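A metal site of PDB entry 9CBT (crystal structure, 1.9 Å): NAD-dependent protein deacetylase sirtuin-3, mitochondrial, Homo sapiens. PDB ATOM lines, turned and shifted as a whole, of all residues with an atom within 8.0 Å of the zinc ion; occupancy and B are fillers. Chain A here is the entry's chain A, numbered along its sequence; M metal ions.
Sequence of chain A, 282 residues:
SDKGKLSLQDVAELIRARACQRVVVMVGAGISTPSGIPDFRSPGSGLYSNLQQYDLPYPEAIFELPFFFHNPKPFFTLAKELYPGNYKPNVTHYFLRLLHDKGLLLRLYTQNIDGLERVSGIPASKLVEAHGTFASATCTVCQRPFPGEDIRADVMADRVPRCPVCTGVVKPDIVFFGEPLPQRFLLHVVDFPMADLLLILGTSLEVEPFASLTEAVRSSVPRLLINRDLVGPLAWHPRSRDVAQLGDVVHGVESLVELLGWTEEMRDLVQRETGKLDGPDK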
ATOM      1  N   THR A 138       8.659 -19.583 -20.348  1.00  0.00           N
ATOM      2  CA  THR A 138       8.089 -18.519 -19.519  1.00  0.00           C
ATOM      3  C   THR A 138       6.712 -18.152 -20.052  1.00  0.00           C
ATOM      4  O   THR A 138       6.521 -18.063 -21.265  1.00  0.00           O
ATOM      5  CB  THR A 138       8.998 -17.282 -19.508  1.00  0.00           C
ATOM      6  OG1 THR A 138      10.346 -17.688 -19.179  1.00  0.00           O
ATOM      7  CG2 THR A 138       8.527 -16.266 -18.473  1.00  0.00           C
ATOM      8  N   CYS A 139       5.764 -17.938 -19.140  1.00  0.00           N
ATOM      9  CA  CYS A 139       4.468 -17.421 -19.522  1.00  0.00           C
ATOM     10  C   CYS A 139       4.615 -15.994 -20.053  1.00  0.00           C
ATOM     11  O   CYS A 139       5.179 -15.129 -19.387  1.00  0.00           O
ATOM     12  CB  CYS A 139       3.504 -17.443 -18.333  1.00  0.00           C
ATOM     13  SG  CYS A 139       1.835 -16.748 -18.635  1.00  0.00           S
ATOM     14  N   THR A 140       4.106 -15.754 -21.262  1.00  0.00           N
ATOM     15  CA  THR A 140       4.165 -14.425 -21.847  1.00  0.00           C
ATOM     16  C   THR A 140       3.309 -13.407 -21.103  1.00  0.00           C
ATOM     17  O   THR A 140       3.413 -12.210 -21.398  1.00  0.00           O
ATOM     18  CB  THR A 140       3.737 -14.461 -23.322  1.00  0.00           C
ATOM     19  OG1 THR A 140       2.433 -15.048 -23.432  1.00  0.00           O
ATOM     20  CG2 THR A 140       4.726 -15.262 -24.146  1.00  0.00           C
ATOM     21  N   VAL A 141       2.475 -13.841 -20.171  1.00  0.00           N
ATOM     22  CA  VAL A 141       1.586 -12.940 -19.434  1.00  0.00           C
ATOM     23  C   VAL A 141       2.101 -12.685 -18.020  1.00  0.00           C
ATOM     24  O   VAL A 141       2.417 -11.546 -17.668  1.00  0.00           O
ATOM     25  CB  VAL A 141       0.135 -13.486 -19.405  1.00  0.00           C
ATOM     26  CG1 VAL A 141      -0.740 -12.555 -18.577  1.00  0.00           C
ATOM     27  CG2 VAL A 141      -0.401 -13.608 -20.822  1.00  0.00           C
ATOM     28  N   CYS A 142       2.191 -13.728 -17.188  1.00  0.00           N
ATOM     29  CA  CYS A 142       2.505 -13.544 -15.784  1.00  0.00           C
ATOM     30  C   CYS A 142       3.992 -13.698 -15.473  1.00  0.00           C
ATOM     31  O   CYS A 142       4.386 -13.550 -14.309  1.00  0.00           O
ATOM     32  CB  CYS A 142       1.682 -14.507 -14.918  1.00  0.00           C
ATOM     33  SG  CYS A 142       2.183 -16.223 -14.955  1.00  0.00           S
ATOM     34  N   GLN A 143       4.818 -14.004 -16.476  1.00  0.00           N
ATOM     35  CA  GLN A 143       6.274 -14.157 -16.374  1.00  0.00           C
ATOM     36  C   GLN A 143       6.700 -15.388 -15.587  1.00  0.00           C
ATOM     37  O   GLN A 143       7.898 -15.543 -15.314  1.00  0.00           O
ATOM     38  CB  GLN A 143       6.956 -12.924 -15.765  1.00  0.00           C
ATOM     39  CG  GLN A 143       6.964 -11.693 -16.657  1.00  0.00           C
ATOM     40  CD  GLN A 143       7.823 -10.564 -16.085  1.00  0.00           C
ATOM     41  OE1 GLN A 143       8.328 -10.663 -14.960  1.00  0.00           O
ATOM     42  NE2 GLN A 143       7.976  -9.489 -16.843  1.00  0.00           N
ATOM     43  N   ARG A 144       5.782 -16.266 -15.212  1.00  0.00           N
ATOM     44  CA  ARG A 144       6.155 -17.443 -14.418  1.00  0.00           C
ATOM     45  C   ARG A 144       7.065 -18.358 -15.231  1.00  0.00           C
ATOM     46  O   ARG A 144       6.786 -18.617 -16.415  1.00  0.00           O
ATOM     47  CB  ARG A 144       4.918 -18.210 -13.948  1.00  0.00           C
ATOM     48  CG  ARG A 144       4.321 -17.671 -12.650  1.00  0.00           C
ATOM     49  CD  ARG A 144       3.103 -18.476 -12.223  1.00  0.00           C
ATOM     50  NE  ARG A 144       2.572 -18.054 -10.926  1.00  0.00           N
ATOM     51  CZ  ARG A 144       1.651 -17.107 -10.765  1.00  0.00           C
ATOM     52  NH1 ARG A 144       1.153 -16.441 -11.796  1.00  0.00           N
ATOM     53  NH2 ARG A 144       1.213 -16.827  -9.539  1.00  0.00           N
ATOM     54  N   PRO A 145       8.147 -18.865 -14.646  1.00  0.00           N
ATOM     55  CA  PRO A 145       9.040 -19.776 -15.375  1.00  0.00           C
ATOM     56  C   PRO A 145       8.626 -21.234 -15.228  1.00  0.00           C
ATOM     57  O   PRO A 145       8.022 -21.644 -14.239  1.00  0.00           O
ATOM     58  CB  PRO A 145      10.390 -19.519 -14.693  1.00  0.00           C
ATOM     59  CG  PRO A 145      10.023 -19.234 -13.271  1.00  0.00           C
ATOM     60  CD  PRO A 145       8.671 -18.542 -13.311  1.00  0.00           C
ATOM     61  N   PHE A 146       8.968 -22.018 -16.250  1.00  0.00           N
ATOM     62  CA  PHE A 146       8.673 -23.443 -16.249  1.00  0.00           C
ATOM     63  C   PHE A 146       9.803 -24.179 -16.938  1.00  0.00           C
ATOM     64  O   PHE A 146      10.432 -23.626 -17.861  1.00  0.00           O
ATOM     65  CB  PHE A 146       7.339 -23.740 -16.960  1.00  0.00           C
ATOM     66  CG  PHE A 146       6.171 -22.967 -16.421  1.00  0.00           C
ATOM     67  CD1 PHE A 146       5.474 -23.419 -15.317  1.00  0.00           C
ATOM     68  CD2 PHE A 146       5.784 -21.776 -17.022  1.00  0.00           C
ATOM     69  CE1 PHE A 146       4.407 -22.703 -14.805  1.00  0.00           C
ATOM     70  CE2 PHE A 146       4.712 -21.049 -16.517  1.00  0.00           C
ATOM     71  CZ  PHE A 146       4.027 -21.513 -15.411  1.00  0.00           C
ATOM     72  N   ARG A 162      -0.317 -23.423 -22.511  1.00  0.00           N
ATOM     73  CA  ARG A 162      -0.903 -22.319 -21.762  1.00  0.00           C
ATOM     74  C   ARG A 162      -0.542 -22.438 -20.292  1.00  0.00           C
ATOM     75  O   ARG A 162      -0.341 -23.534 -19.759  1.00  0.00           O
ATOM     76  CB  ARG A 162      -2.418 -22.286 -21.929  1.00  0.00           C
ATOM     77  CG  ARG A 162      -2.857 -22.374 -23.380  1.00  0.00           C
ATOM     78  CD  ARG A 162      -4.268 -21.866 -23.555  1.00  0.00           C
ATOM     79  NE  ARG A 162      -4.321 -20.407 -23.466  1.00  0.00           N
ATOM     80  CZ  ARG A 162      -4.321 -19.604 -24.514  1.00  0.00           C
ATOM     81  NH1 ARG A 162      -4.303 -20.086 -25.748  1.00  0.00           N
ATOM     82  NH2 ARG A 162      -4.346 -18.288 -24.321  1.00  0.00           N
ATOM     83  N   CYS A 163      -0.471 -21.274 -19.641  1.00  0.00           N
ATOM     84  CA  CYS A 163       0.003 -21.193 -18.263  1.00  0.00           C
ATOM     85  C   CYS A 163      -0.966 -21.908 -17.321  1.00  0.00           C
ATOM     86  O   CYS A 163      -2.176 -21.652 -17.365  1.00  0.00           O
ATOM     87  CB  CYS A 163       0.144 -19.720 -17.864  1.00  0.00           C
ATOM     88  SG  CYS A 163       0.686 -19.420 -16.195  1.00  0.00           S
ATOM     89  N   PRO A 164      -0.475 -22.799 -16.453  1.00  0.00           N
ATOM     90  CA  PRO A 164      -1.394 -23.505 -15.544  1.00  0.00           C
ATOM     91  C   PRO A 164      -1.998 -22.610 -14.488  1.00  0.00           C
ATOM     92  O   PRO A 164      -2.947 -23.029 -13.818  1.00  0.00           O
ATOM     93  CB  PRO A 164      -0.492 -24.584 -14.915  1.00  0.00           C
ATOM     94  CG  PRO A 164       0.877 -24.055 -15.013  1.00  0.00           C
ATOM     95  CD  PRO A 164       0.928 -23.198 -16.257  1.00  0.00           C
ATOM     96  N   VAL A 165      -1.487 -21.402 -14.315  1.00  0.00           N
ATOM     97  CA  VAL A 165      -2.007 -20.467 -13.333  1.00  0.00           C
ATOM     98  C   VAL A 165      -2.968 -19.454 -13.957  1.00  0.00           C
ATOM     99  O   VAL A 165      -4.088 -19.275 -13.481  1.00  0.00           O
ATOM    100  CB  VAL A 165      -0.854 -19.775 -12.587  1.00  0.00           C
ATOM    101  CG1 VAL A 165      -1.402 -18.801 -11.558  1.00  0.00           C
ATOM    102  CG2 VAL A 165       0.038 -20.815 -11.922  1.00  0.00           C
ATOM    103  N   CYS A 166      -2.557 -18.806 -15.048  1.00  0.00           N
ATOM    104  CA  CYS A 166      -3.317 -17.696 -15.609  1.00  0.00           C
ATOM    105  C   CYS A 166      -3.803 -17.913 -17.036  1.00  0.00           C
ATOM    106  O   CYS A 166      -4.484 -17.034 -17.575  1.00  0.00           O
ATOM    107  CB  CYS A 166      -2.475 -16.407 -15.556  1.00  0.00           C
ATOM    108  SG  CYS A 166      -1.246 -16.234 -16.897  1.00  0.00           S
ATOM    109  N   THR A 167      -3.480 -19.055 -17.654  1.00  0.00           N
ATOM    110  CA  THR A 167      -3.837 -19.472 -19.004  1.00  0.00           C
ATOM    111  C   THR A 167      -3.087 -18.714 -20.096  1.00  0.00           C
ATOM    112  O   THR A 167      -3.354 -18.943 -21.283  1.00  0.00           O
ATOM    113  CB  THR A 167      -5.342 -19.356 -19.321  1.00  0.00           C
ATOM    114  OG1 THR A 167      -5.667 -17.974 -19.547  1.00  0.00           O
ATOM    115  CG2 THR A 167      -6.179 -19.908 -18.189  1.00  0.00           C
ATOM    116  N   GLY A 168      -2.161 -17.823 -19.737  1.00  0.00           N
ATOM    117  CA  GLY A 168      -1.384 -17.135 -20.749  1.00  0.00           C
ATOM    118  C   GLY A 168      -0.577 -18.110 -21.587  1.00  0.00           C
ATOM    119  O   GLY A 168      -0.234 -19.210 -21.149  1.00  0.00           O
ATOM    120  N   VAL A 169      -0.323 -17.715 -22.831  1.00  0.00           N
ATOM    121  CA  VAL A 169       0.505 -18.526 -23.718  1.00  0.00           C
ATOM    122  C   VAL A 169       1.908 -18.595 -23.157  1.00  0.00           C
ATOM    123  O   VAL A 169       2.518 -17.570 -22.847  1.00  0.00           O
ATOM    124  CB  VAL A 169       0.502 -17.950 -25.139  1.00  0.00           C
ATOM    125  CG1 VAL A 169       1.463 -18.732 -26.025  1.00  0.00           C
ATOM    126  CG2 VAL A 169      -0.904 -17.968 -25.735  1.00  0.00           C
ATOM    127  N   VAL A 170       2.438 -19.815 -23.029  1.00  0.00           N
ATOM    128  CA  VAL A 170       3.784 -20.026 -22.513  1.00  0.00           C
ATOM    129  C   VAL A 170       4.743 -20.147 -23.684  1.00  0.00           C
ATOM    130  O   VAL A 170       4.504 -20.925 -24.623  1.00  0.00           O
ATOM    131  CB  VAL A 170       3.846 -21.274 -21.621  1.00  0.00           C
ATOM    132  CG1 VAL A 170       5.294 -21.555 -21.219  1.00  0.00           C
ATOM    133  CG2 VAL A 170       2.983 -21.078 -20.381  1.00  0.00           C
HETATM  134 ZN    ZN M   1       0.846 -17.140 -16.581  1.00  0.00          ZN
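Four residues have an atom within 4 Å of the zinc ion: Cys 139, Cys 142, Cys 163 and Cys 166.
Along chain A the residues within 4 Å of the zinc ion span positions 139 to 166.
The nearest printed residue that does not touch the zinc ion is Gly 168 (4.4 Å).
The guanidinium group (NH1) of Arg 144 sits close to the side-chain sulfur (SG) of Cys 142 (3.3 Å).
The side-chain sulfur of Cys 166 sits close to the backbone NH of Gly 168, 3.4 Å away.
N of Val 141 sits close to SG of Cys 139.
The backbone NH of Cys 139 lies within hydrogen-bond range of the backbone carbonyl oxygen of Arg 144, at 3.0 Å.
N of Cys 163 lies within hydrogen-bond range of O of Gly 168, at 2.6 Å.
SG of Cys 163 sits close to N of Val 165, at 3.5 Å.
The zinc ion is bound by SG of Cys 142 (2.3 Å).
The side-chain sulfur (SG) of Cys 166 binds the zinc ion (2.3 Å).
The zinc ion is bound by SG of Cys 139, 2.3 Å away.
The side-chain sulfur (SG) of Cys 163 is bound to the zinc ion (2.3 Å).
The zinc ion has four donor atoms within binding distance.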
